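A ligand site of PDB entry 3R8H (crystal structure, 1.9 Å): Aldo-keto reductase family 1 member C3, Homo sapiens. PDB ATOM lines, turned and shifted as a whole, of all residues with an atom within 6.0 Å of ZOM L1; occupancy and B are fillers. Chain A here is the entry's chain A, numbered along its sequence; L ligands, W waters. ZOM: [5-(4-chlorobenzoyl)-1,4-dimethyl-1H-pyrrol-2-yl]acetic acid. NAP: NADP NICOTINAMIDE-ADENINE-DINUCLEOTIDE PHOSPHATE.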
ATOM      1  N   TYR A  24      29.997 -19.629 -20.102  1.00  0.00           N
ATOM      2  CA  TYR A  24      29.083 -20.102 -21.120  1.00  0.00           C
ATOM      3  C   TYR A  24      29.325 -19.346 -22.422  1.00  0.00           C
ATOM      4  O   TYR A  24      29.506 -18.126 -22.414  1.00  0.00           O
ATOM      5  CB  TYR A  24      27.605 -19.939 -20.724  1.00  0.00           C
ATOM      6  CG  TYR A  24      26.694 -20.396 -21.876  1.00  0.00           C
ATOM      7  CD1 TYR A  24      26.544 -21.769 -22.120  1.00  0.00           C
ATOM      8  CD2 TYR A  24      26.089 -19.482 -22.777  1.00  0.00           C
ATOM      9  CE1 TYR A  24      25.798 -22.271 -23.164  1.00  0.00           C
ATOM     10  CE2 TYR A  24      25.240 -20.013 -23.886  1.00  0.00           C
ATOM     11  CZ  TYR A  24      25.118 -21.381 -24.029  1.00  0.00           C
ATOM     12  OH  TYR A  24      24.381 -21.932 -25.031  1.00  0.00           O
ATOM     13  N   ALA A  52      28.903 -25.381 -15.628  1.00  0.00           N
ATOM     14  CA  ALA A  52      27.661 -26.085 -15.440  1.00  0.00           C
ATOM     15  C   ALA A  52      27.677 -27.270 -16.366  1.00  0.00           C
ATOM     16  O   ALA A  52      28.280 -27.204 -17.466  1.00  0.00           O
ATOM     17  CB  ALA A  52      26.373 -25.187 -15.846  1.00  0.00           C
ATOM     18  N   LEU A  54      25.240 -28.085 -18.252  1.00  0.00           N
ATOM     19  CA  LEU A  54      24.678 -27.590 -19.496  1.00  0.00           C
ATOM     20  C   LEU A  54      25.659 -26.990 -20.517  1.00  0.00           C
ATOM     21  O   LEU A  54      25.353 -26.992 -21.727  1.00  0.00           O
ATOM     22  CB  LEU A  54      23.695 -26.465 -19.168  1.00  0.00           C
ATOM     23  CG  LEU A  54      22.761 -25.973 -20.310  1.00  0.00           C
ATOM     24  CD1 LEU A  54      21.766 -27.070 -20.825  1.00  0.00           C
ATOM     25  CD2 LEU A  54      22.059 -24.662 -19.950  1.00  0.00           C
ATOM     26  N   TYR A  55      26.768 -26.400 -20.069  1.00  0.00           N
ATOM     27  CA  TYR A  55      27.564 -25.553 -20.933  1.00  0.00           C
ATOM     28  C   TYR A  55      28.418 -26.415 -21.844  1.00  0.00           C
ATOM     29  O   TYR A  55      29.031 -25.908 -22.792  1.00  0.00           O
ATOM     30  CB  TYR A  55      28.466 -24.688 -20.036  1.00  0.00           C
ATOM     31  CG  TYR A  55      27.690 -23.753 -19.140  1.00  0.00           C
ATOM     32  CD1 TYR A  55      26.265 -23.623 -19.234  1.00  0.00           C
ATOM     33  CD2 TYR A  55      28.364 -22.987 -18.202  1.00  0.00           C
ATOM     34  CE1 TYR A  55      25.580 -22.719 -18.337  1.00  0.00           C
ATOM     35  CE2 TYR A  55      27.676 -22.127 -17.304  1.00  0.00           C
ATOM     36  CZ  TYR A  55      26.291 -22.016 -17.401  1.00  0.00           C
ATOM     37  OH  TYR A  55      25.688 -21.155 -16.522  1.00  0.00           O
ATOM     38  N   LYS A  84      26.803 -26.885 -11.833  1.00  0.00           N
ATOM     39  CA  LYS A  84      25.354 -26.748 -11.636  1.00  0.00           C
ATOM     40  C   LYS A  84      24.680 -28.031 -12.122  1.00  0.00           C
ATOM     41  O   LYS A  84      25.017 -28.594 -13.183  1.00  0.00           O
ATOM     42  CB  LYS A  84      24.740 -25.564 -12.447  1.00  0.00           C
ATOM     43  CG  LYS A  84      25.505 -24.276 -12.223  1.00  0.00           C
ATOM     44  CD  LYS A  84      24.704 -23.039 -12.768  1.00  0.00           C
ATOM     45  CE  LYS A  84      25.645 -21.752 -12.731  1.00  0.00           C
ATOM     46  NZ  LYS A  84      26.592 -21.687 -13.913  1.00  0.00           N
ATOM     47  N   TRP A  86      21.694 -29.780 -13.823  1.00  0.00           N
ATOM     48  CA  TRP A  86      20.750 -29.379 -14.827  1.00  0.00           C
ATOM     49  C   TRP A  86      19.368 -29.944 -14.428  1.00  0.00           C
ATOM     50  O   TRP A  86      19.263 -30.888 -13.622  1.00  0.00           O
ATOM     51  CB  TRP A  86      21.200 -29.890 -16.225  1.00  0.00           C
ATOM     52  CG  TRP A  86      20.271 -29.334 -17.299  1.00  0.00           C
ATOM     53  CD1 TRP A  86      19.526 -30.080 -18.202  1.00  0.00           C
ATOM     54  CD2 TRP A  86      19.871 -27.967 -17.471  1.00  0.00           C
ATOM     55  NE1 TRP A  86      18.670 -29.234 -18.916  1.00  0.00           N
ATOM     56  CE2 TRP A  86      18.881 -27.936 -18.485  1.00  0.00           C
ATOM     57  CE3 TRP A  86      20.223 -26.764 -16.834  1.00  0.00           C
ATOM     58  CZ2 TRP A  86      18.291 -26.741 -18.916  1.00  0.00           C
ATOM     59  CZ3 TRP A  86      19.624 -25.555 -17.272  1.00  0.00           C
ATOM     60  CH2 TRP A  86      18.654 -25.575 -18.310  1.00  0.00           C
ATOM     61  N   HIS A 117      20.547 -25.578 -10.931  1.00  0.00           N
ATOM     62  CA  HIS A 117      20.720 -24.556 -11.983  1.00  0.00           C
ATOM     63  C   HIS A 117      19.433 -23.733 -12.104  1.00  0.00           C
ATOM     64  O   HIS A 117      19.460 -22.513 -12.413  1.00  0.00           O
ATOM     65  CB  HIS A 117      21.085 -25.220 -13.338  1.00  0.00           C
ATOM     66  CG  HIS A 117      21.773 -24.313 -14.321  1.00  0.00           C
ATOM     67  ND1 HIS A 117      22.725 -24.780 -15.211  1.00  0.00           N
ATOM     68  CD2 HIS A 117      21.548 -23.022 -14.669  1.00  0.00           C
ATOM     69  CE1 HIS A 117      23.112 -23.801 -15.997  1.00  0.00           C
ATOM     70  NE2 HIS A 117      22.392 -22.722 -15.722  1.00  0.00           N
ATOM     71  N   SER A 118      18.291 -24.400 -11.945  1.00  0.00           N
ATOM     72  CA  SER A 118      17.074 -23.637 -12.004  1.00  0.00           C
ATOM     73  C   SER A 118      15.947 -24.425 -11.306  1.00  0.00           C
ATOM     74  O   SER A 118      16.035 -25.665 -11.155  1.00  0.00           O
ATOM     75  CB  SER A 118      16.784 -23.380 -13.510  1.00  0.00           C
ATOM     76  OG  SER A 118      15.470 -23.510 -13.881  1.00  0.00           O
ATOM     77  N   MET A 120      13.087 -24.926 -12.531  1.00  0.00           N
ATOM     78  CA  MET A 120      12.083 -25.382 -13.514  1.00  0.00           C
ATOM     79  C   MET A 120      12.348 -26.805 -13.970  1.00  0.00           C
ATOM     80  O   MET A 120      12.949 -27.033 -14.987  1.00  0.00           O
ATOM     81  CB  MET A 120      12.044 -24.404 -14.738  1.00  0.00           C
ATOM     82  CG  MET A 120      11.325 -23.100 -14.355  1.00  0.00           C
ATOM     83  SD  MET A 120      11.629 -21.775 -15.491  1.00  0.00           S
ATOM     84  CE  MET A 120      13.266 -21.298 -15.019  1.00  0.00           C
ATOM     85  N   ASN A 167      18.385 -19.090  -9.919  1.00  0.00           N
ATOM     86  CA  ASN A 167      17.104 -18.715 -10.537  1.00  0.00           C
ATOM     87  C   ASN A 167      15.938 -18.974  -9.619  1.00  0.00           C
ATOM     88  O   ASN A 167      14.781 -19.165 -10.105  1.00  0.00           O
ATOM     89  CB  ASN A 167      16.914 -19.448 -11.875  1.00  0.00           C
ATOM     90  CG  ASN A 167      17.921 -18.988 -12.903  1.00  0.00           C
ATOM     91  OD1 ASN A 167      17.976 -17.814 -13.207  1.00  0.00           O
ATOM     92  ND2 ASN A 167      18.789 -19.896 -13.333  1.00  0.00           N
ATOM     93  N   GLN A 190      22.095 -17.599  -7.380  1.00  0.00           N
ATOM     94  CA  GLN A 190      22.612 -16.976  -8.588  1.00  0.00           C
ATOM     95  C   GLN A 190      21.448 -16.669  -9.521  1.00  0.00           C
ATOM     96  O   GLN A 190      20.725 -17.569  -9.986  1.00  0.00           O
ATOM     97  CB  GLN A 190      23.563 -17.927  -9.265  1.00  0.00           C
ATOM     98  CG  GLN A 190      24.241 -17.275 -10.506  1.00  0.00           C
ATOM     99  CD  GLN A 190      25.200 -18.258 -11.200  1.00  0.00           C
ATOM    100  OE1 GLN A 190      26.177 -18.810 -10.576  1.00  0.00           O
ATOM    101  NE2 GLN A 190      24.999 -18.462 -12.504  1.00  0.00           N
ATOM    102  N   GLU A 192      19.617 -13.550 -12.476  1.00  0.00           N
ATOM    103  CA  GLU A 192      19.847 -12.511 -13.458  1.00  0.00           C
ATOM    104  C   GLU A 192      19.790 -11.219 -12.660  1.00  0.00           C
ATOM    105  O   GLU A 192      18.838 -10.979 -11.916  1.00  0.00           O
ATOM    106  CB  GLU A 192      18.756 -12.503 -14.477  1.00  0.00           C
ATOM    107  CG  GLU A 192      19.102 -11.429 -15.547  1.00  0.00           C
ATOM    108  CD  GLU A 192      18.182 -11.414 -16.773  1.00  0.00           C
ATOM    109  OE1 GLU A 192      17.607 -12.454 -17.287  1.00  0.00           O
ATOM    110  OE2 GLU A 192      18.077 -10.296 -17.283  1.00  0.00           O
ATOM    111  N   TYR A 216      24.211 -12.939 -12.590  1.00  0.00           N
ATOM    112  CA  TYR A 216      24.623 -13.265 -13.962  1.00  0.00           C
ATOM    113  C   TYR A 216      23.909 -12.299 -14.935  1.00  0.00           C
ATOM    114  O   TYR A 216      22.952 -11.609 -14.567  1.00  0.00           O
ATOM    115  CB  TYR A 216      24.322 -14.728 -14.323  1.00  0.00           C
ATOM    116  CG  TYR A 216      22.852 -15.104 -14.498  1.00  0.00           C
ATOM    117  CD1 TYR A 216      22.117 -14.636 -15.604  1.00  0.00           C
ATOM    118  CD2 TYR A 216      22.227 -15.979 -13.615  1.00  0.00           C
ATOM    119  CE1 TYR A 216      20.778 -15.088 -15.793  1.00  0.00           C
ATOM    120  CE2 TYR A 216      20.877 -16.434 -13.797  1.00  0.00           C
ATOM    121  CZ  TYR A 216      20.183 -15.968 -14.882  1.00  0.00           C
ATOM    122  OH  TYR A 216      18.879 -16.378 -15.142  1.00  0.00           O
ATOM    123  N   GLN A 222      24.360 -12.213 -23.217  1.00  0.00           N
ATOM    124  CA  GLN A 222      24.941 -12.378 -24.555  1.00  0.00           C
ATOM    125  C   GLN A 222      23.902 -12.141 -25.642  1.00  0.00           C
ATOM    126  O   GLN A 222      24.205 -12.263 -26.846  1.00  0.00           O
ATOM    127  CB  GLN A 222      25.577 -13.764 -24.693  1.00  0.00           C
ATOM    128  CG  GLN A 222      26.623 -13.943 -23.550  1.00  0.00           C
ATOM    129  CD  GLN A 222      27.458 -15.229 -23.733  1.00  0.00           C
ATOM    130  OE1 GLN A 222      27.835 -15.563 -24.880  1.00  0.00           O
ATOM    131  NE2 GLN A 222      27.653 -15.978 -22.646  1.00  0.00           N
ATOM    132  N   TRP A 227      16.527 -16.880 -26.922  1.00  0.00           N
ATOM    133  CA  TRP A 227      15.656 -16.465 -25.775  1.00  0.00           C
ATOM    134  C   TRP A 227      15.630 -15.007 -25.367  1.00  0.00           C
ATOM    135  O   TRP A 227      14.856 -14.645 -24.475  1.00  0.00           O
ATOM    136  CB  TRP A 227      15.913 -17.334 -24.537  1.00  0.00           C
ATOM    137  CG  TRP A 227      17.329 -17.201 -23.994  1.00  0.00           C
ATOM    138  CD1 TRP A 227      17.835 -16.220 -23.172  1.00  0.00           C
ATOM    139  CD2 TRP A 227      18.384 -18.151 -24.201  1.00  0.00           C
ATOM    140  NE1 TRP A 227      19.177 -16.474 -22.894  1.00  0.00           N
ATOM    141  CE2 TRP A 227      19.530 -17.648 -23.526  1.00  0.00           C
ATOM    142  CE3 TRP A 227      18.493 -19.346 -24.936  1.00  0.00           C
ATOM    143  CZ2 TRP A 227      20.771 -18.342 -23.542  1.00  0.00           C
ATOM    144  CZ3 TRP A 227      19.699 -20.020 -24.941  1.00  0.00           C
ATOM    145  CH2 TRP A 227      20.827 -19.512 -24.279  1.00  0.00           C
ATOM    146  N   PHE A 306      16.264 -12.836 -20.354  1.00  0.00           N
ATOM    147  CA  PHE A 306      15.525 -14.095 -20.630  1.00  0.00           C
ATOM    148  C   PHE A 306      14.027 -13.824 -20.747  1.00  0.00           C
ATOM    149  O   PHE A 306      13.401 -13.403 -19.773  1.00  0.00           O
ATOM    150  CB  PHE A 306      15.647 -15.217 -19.569  1.00  0.00           C
ATOM    151  CG  PHE A 306      14.712 -16.398 -19.931  1.00  0.00           C
ATOM    152  CD1 PHE A 306      13.362 -16.436 -19.513  1.00  0.00           C
ATOM    153  CD2 PHE A 306      15.174 -17.344 -20.814  1.00  0.00           C
ATOM    154  CE1 PHE A 306      12.491 -17.473 -19.941  1.00  0.00           C
ATOM    155  CE2 PHE A 306      14.333 -18.414 -21.309  1.00  0.00           C
ATOM    156  CZ  PHE A 306      13.005 -18.453 -20.857  1.00  0.00           C
ATOM    157  N   PHE A 311       9.977 -21.214 -21.423  1.00  0.00           N
ATOM    158  CA  PHE A 311       9.835 -21.411 -19.968  1.00  0.00           C
ATOM    159  C   PHE A 311       8.867 -20.518 -19.281  1.00  0.00           C
ATOM    160  O   PHE A 311       8.582 -20.746 -18.115  1.00  0.00           O
ATOM    161  CB  PHE A 311      11.184 -21.339 -19.238  1.00  0.00           C
ATOM    162  CG  PHE A 311      12.121 -22.441 -19.679  1.00  0.00           C
ATOM    163  CD1 PHE A 311      11.796 -23.803 -19.390  1.00  0.00           C
ATOM    164  CD2 PHE A 311      13.269 -22.151 -20.406  1.00  0.00           C
ATOM    165  CE1 PHE A 311      12.602 -24.839 -19.888  1.00  0.00           C
ATOM    166  CE2 PHE A 311      14.111 -23.188 -20.891  1.00  0.00           C
ATOM    167  CZ  PHE A 311      13.783 -24.532 -20.624  1.00  0.00           C
ATOM    168  N   TYR A 317       8.223 -21.153 -13.065  1.00  0.00           N
ATOM    169  CA  TYR A 317       8.861 -19.969 -13.655  1.00  0.00           C
ATOM    170  C   TYR A 317       9.107 -18.955 -12.555  1.00  0.00           C
ATOM    171  O   TYR A 317       8.171 -18.529 -11.891  1.00  0.00           O
ATOM    172  CB  TYR A 317       7.881 -19.383 -14.671  1.00  0.00           C
ATOM    173  CG  TYR A 317       8.389 -18.189 -15.428  1.00  0.00           C
ATOM    174  CD1 TYR A 317       9.601 -18.250 -16.163  1.00  0.00           C
ATOM    175  CD2 TYR A 317       7.657 -17.013 -15.455  1.00  0.00           C
ATOM    176  CE1 TYR A 317      10.052 -17.147 -16.894  1.00  0.00           C
ATOM    177  CE2 TYR A 317       8.136 -15.884 -16.170  1.00  0.00           C
ATOM    178  CZ  TYR A 317       9.313 -15.979 -16.882  1.00  0.00           C
ATOM    179  OH  TYR A 317       9.762 -14.925 -17.588  1.00  0.00           O
ATOM    180  N   PRO A 318      10.347 -18.509 -12.385  1.00  0.00           N
ATOM    181  CA  PRO A 318      10.489 -17.657 -11.218  1.00  0.00           C
ATOM    182  C   PRO A 318       9.990 -16.249 -11.372  1.00  0.00           C
ATOM    183  O   PRO A 318       9.827 -15.608 -10.353  1.00  0.00           O
ATOM    184  CB  PRO A 318      12.024 -17.596 -11.004  1.00  0.00           C
ATOM    185  CG  PRO A 318      12.585 -17.838 -12.400  1.00  0.00           C
ATOM    186  CD  PRO A 318      11.658 -18.951 -12.900  1.00  0.00           C
ATOM    187  N   TYR A 319       9.769 -15.744 -12.588  1.00  0.00           N
ATOM    188  CA  TYR A 319       9.373 -14.331 -12.715  1.00  0.00           C
ATOM    189  C   TYR A 319       7.820 -14.180 -12.629  1.00  0.00           C
ATOM    190  O   TYR A 319       7.305 -13.094 -12.775  1.00  0.00           O
ATOM    191  CB  TYR A 319       9.902 -13.711 -14.026  1.00  0.00           C
ATOM    192  CG  TYR A 319      11.421 -13.817 -14.126  1.00  0.00           C
ATOM    193  CD1 TYR A 319      12.191 -13.650 -12.980  1.00  0.00           C
ATOM    194  CD2 TYR A 319      12.042 -14.116 -15.312  1.00  0.00           C
ATOM    195  CE1 TYR A 319      13.588 -13.728 -13.023  1.00  0.00           C
ATOM    196  CE2 TYR A 319      13.460 -14.199 -15.380  1.00  0.00           C
ATOM    197  CZ  TYR A 319      14.221 -14.022 -14.216  1.00  0.00           C
ATOM    198  OH  TYR A 319      15.644 -14.172 -14.229  1.00  0.00           O
HETATM  199 CL   ZOM L   1      13.503 -17.455 -15.893  1.00  0.00          CL
HETATM  200  N1  ZOM L   1      20.470 -20.686 -18.851  1.00  0.00           N
HETATM  201  C2  ZOM L   1      21.411 -19.807 -19.570  1.00  0.00           C
HETATM  202  C3  ZOM L   1      20.806 -18.574 -19.669  1.00  0.00           C
HETATM  203  C4  ZOM L   1      19.535 -18.662 -19.183  1.00  0.00           C
HETATM  204  C5  ZOM L   1      19.263 -19.942 -18.689  1.00  0.00           C
HETATM  205  C6  ZOM L   1      18.018 -20.615 -18.057  1.00  0.00           C
HETATM  206  O6  ZOM L   1      17.867 -21.829 -18.192  1.00  0.00           O
HETATM  207  C7  ZOM L   1      22.791 -20.316 -19.975  1.00  0.00           C
HETATM  208  C8  ZOM L   1      23.716 -20.094 -18.751  1.00  0.00           C
HETATM  209  C9  ZOM L   1      20.580 -22.157 -18.560  1.00  0.00           C
HETATM  210  OH  ZOM L   1      24.729 -19.402 -19.028  1.00  0.00           O
HETATM  211  C10 ZOM L   1      18.530 -17.492 -19.080  1.00  0.00           C
HETATM  212  C1B ZOM L   1      16.921 -19.796 -17.513  1.00  0.00           C
HETATM  213  C2B ZOM L   1      15.690 -19.964 -18.154  1.00  0.00           C
HETATM  214  C3B ZOM L   1      14.655 -19.165 -17.579  1.00  0.00           C
HETATM  215  C4B ZOM L   1      14.841 -18.355 -16.488  1.00  0.00           C
HETATM  216  C5B ZOM L   1      16.088 -18.174 -15.857  1.00  0.00           C
HETATM  217  C6B ZOM L   1      17.134 -18.955 -16.392  1.00  0.00           C
HETATM  218  OXT ZOM L   1      23.491 -20.728 -17.627  1.00  0.00           O
HETATM  219  PA  NAP L   2      27.507 -11.321 -19.355  1.00  0.00           P
HETATM  220  O1A NAP L   2      28.487 -11.448 -18.217  1.00  0.00           O
HETATM  221  O2A NAP L   2      26.293 -10.449 -19.082  1.00  0.00           O
HETATM  222  O5B NAP L   2      28.343 -10.693 -20.582  1.00  0.00           O
HETATM  223  C5B NAP L   2      27.576 -10.207 -21.714  1.00  0.00           C
HETATM  224  C4B NAP L   2      28.618  -9.844 -22.861  1.00  0.00           C
HETATM  225  O4B NAP L   2      29.445  -8.838 -22.261  1.00  0.00           O
HETATM  226  C3B NAP L   2      29.585 -10.994 -23.107  1.00  0.00           C
HETATM  227  O3B NAP L   2      29.208 -11.885 -24.156  1.00  0.00           O
HETATM  228  C2B NAP L   2      30.944 -10.305 -23.395  1.00  0.00           C
HETATM  229  O2B NAP L   2      31.225 -10.358 -24.823  1.00  0.00           O
HETATM  230  C1B NAP L   2      30.651  -8.865 -23.040  1.00  0.00           C
HETATM  231  N9A NAP L   2      31.712  -8.154 -22.225  1.00  0.00           N
HETATM  232  C8A NAP L   2      32.416  -8.740 -21.255  1.00  0.00           C
HETATM  233  N7A NAP L   2      33.260  -7.843 -20.727  1.00  0.00           N
HETATM  234  C5A NAP L   2      33.081  -6.690 -21.427  1.00  0.00           C
HETATM  235  C6A NAP L   2      33.712  -5.446 -21.404  1.00  0.00           C
HETATM  236  N6A NAP L   2      34.658  -5.149 -20.432  1.00  0.00           N
HETATM  237  N1A NAP L   2      33.270  -4.519 -22.316  1.00  0.00           N
HETATM  238  C2A NAP L   2      32.327  -4.735 -23.242  1.00  0.00           C
HETATM  239  N3A NAP L   2      31.718  -5.954 -23.340  1.00  0.00           N
HETATM  240  C4A NAP L   2      32.126  -6.919 -22.417  1.00  0.00           C
HETATM  241  O3  NAP L   2      27.043 -12.803 -20.028  1.00  0.00           O
HETATM  242  PN  NAP L   2      26.177 -13.956 -19.420  1.00  0.00           P
HETATM  243  O1N NAP L   2      26.621 -15.135 -20.160  1.00  0.00           O
HETATM  244  O2N NAP L   2      24.768 -13.617 -19.594  1.00  0.00           O
HETATM  245  O5D NAP L   2      26.392 -14.011 -17.815  1.00  0.00           O
HETATM  246  C5D NAP L   2      27.707 -14.448 -17.352  1.00  0.00           C
HETATM  247  C4D NAP L   2      27.824 -15.902 -16.839  1.00  0.00           C
HETATM  248  O4D NAP L   2      26.840 -16.091 -15.861  1.00  0.00           O
HETATM  249  C3D NAP L   2      27.568 -17.040 -17.874  1.00  0.00           C
HETATM  250  O3D NAP L   2      28.699 -17.177 -18.759  1.00  0.00           O
HETATM  251  C2D NAP L   2      27.324 -18.214 -16.944  1.00  0.00           C
HETATM  252  O2D NAP L   2      28.615 -18.572 -16.369  1.00  0.00           O
HETATM  253  C1D NAP L   2      26.467 -17.483 -15.864  1.00  0.00           C
HETATM  254  N1N NAP L   2      25.004 -17.544 -16.197  1.00  0.00           N
HETATM  255  C2N NAP L   2      24.262 -18.384 -15.381  1.00  0.00           C
HETATM  256  C3N NAP L   2      22.891 -18.519 -15.667  1.00  0.00           C
HETATM  257  C7N NAP L   2      22.072 -19.427 -14.776  1.00  0.00           C
HETATM  258  O7N NAP L   2      20.972 -19.841 -15.158  1.00  0.00           O
HETATM  259  N7N NAP L   2      22.551 -19.622 -13.501  1.00  0.00           N
HETATM  260  C4N NAP L   2      22.292 -17.845 -16.753  1.00  0.00           C
HETATM  261  C5N NAP L   2      23.058 -16.988 -17.549  1.00  0.00           C
HETATM  262  C6N NAP L   2      24.398 -16.808 -17.314  1.00  0.00           C
HETATM  263  P2B NAP L   2      32.731 -10.891 -25.263  1.00  0.00           P
HETATM  264  O1X NAP L   2      32.819 -12.360 -24.923  1.00  0.00           O
HETATM  265  O2X NAP L   2      32.838 -10.604 -26.778  1.00  0.00           O
HETATM  266  O3X NAP L   2      33.818 -10.044 -24.524  1.00  0.00           O
HETATM  267  O   HOH W   1      24.795 -17.285 -20.673  1.00  0.00           O
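Water W1 lies within hydrogen-bond range of OH of ZOM L1 (2.7 Å) and O1N of NAP L2 (2.9 Å).
NZ of Lys 84 lies within hydrogen-bond range of OH of Tyr 55. O of His 117 sits at hydrogen-bond distance from ND2 of Asn 167 (2.9 Å). The side-chain amide oxygen (OD1) of Asn 167 sits at hydrogen-bond distance from the side-chain hydroxyl (OH) of Tyr 216 (2.6 Å). O of Gln 190 sits at hydrogen-bond distance from N of Asn 167, 2.8 Å away. NE2 of Gln 222 sits at hydrogen-bond distance from O of Tyr 24 (2.8 Å). The backbone NH of Phe 306 is in hydrogen-bond range of the side-chain carboxylate of Glu 192 (3.4 Å). N of Met 120 lies within hydrogen-bond range of OG of Ser 118, 3.1 Å away.
CB of Tyr 24 touches OH of ZOM L1 (3.4 Å). Leu 54 touches ZOM L1. CZ3 of Trp 86 touches C9 of ZOM L1, at 3.8 Å. Met 120 touches ZOM L1. OD1 of Asn 167 touches C5B of ZOM L1, at 3.3 Å. OH of Tyr 216 touches C6B of ZOM L1, at 3.4 Å. CZ2 of Trp 227 touches C3 of ZOM L1, at 3.9 Å. CD1 of Phe 306 touches C3B of ZOM L1, 3.6 Å away. Phe 311 touches ZOM L1 (CD2 to C2B, 3.96 Å). CE1 of Tyr 317 touches CL of ZOM L1, at 3.6 Å. CG of Pro 318 touches CL of ZOM L1, 3.6 Å away. CE2 of Tyr 319 touches CL of ZOM L1 (3.3 Å). Hydrophobic or aromatic side chains within 4 Å of ZOM L1: Tyr 24, Leu 54, Tyr 55, Trp 86, His 117, Met 120, Trp 227, Phe 306, Phe 311, Tyr 317, Pro 318 and Tyr 319. 14 residues have an atom within 4 Å of ZOM L1: Tyr 24, Leu 54, Tyr 55, Trp 86, His 117, Met 120, Asn 167, Tyr 216, Trp 227, Phe 306, Phe 311, Tyr 317, Pro 318 and Tyr 319. The nearest printed residue that does not touch ZOM L1 is Lys 84 (4.9 Å).
The side-chain hydroxyl (OH) of Tyr 55 lies within hydrogen-bond range of an oxygen (OXT) of ZOM L1, 2.5 Å away. OXT of ZOM L1 lies within hydrogen-bond range of NE2 of His 117 (3.0 Å). A ring nitrogen (NE2) of His 117 is in hydrogen-bond range of an oxygen (O7N) of NAP L2 (3.3 Å). An oxygen (O7N) of NAP L2 lies within hydrogen-bond range of the side-chain amide nitrogen (ND2) of Asn 167 (2.8 Å). O3D of NAP L2 lies within hydrogen-bond range of N of Tyr 24, 3.1 Å away. An oxygen (O1N) of NAP L2 is in hydrogen-bond range of the side-chain amide nitrogen (NE2) of Gln 222, at 2.8 Å. A nitrogen (N7N) of NAP L2 lies close to the side-chain amide nitrogen (NE2) of Gln 190 (2.9 Å).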
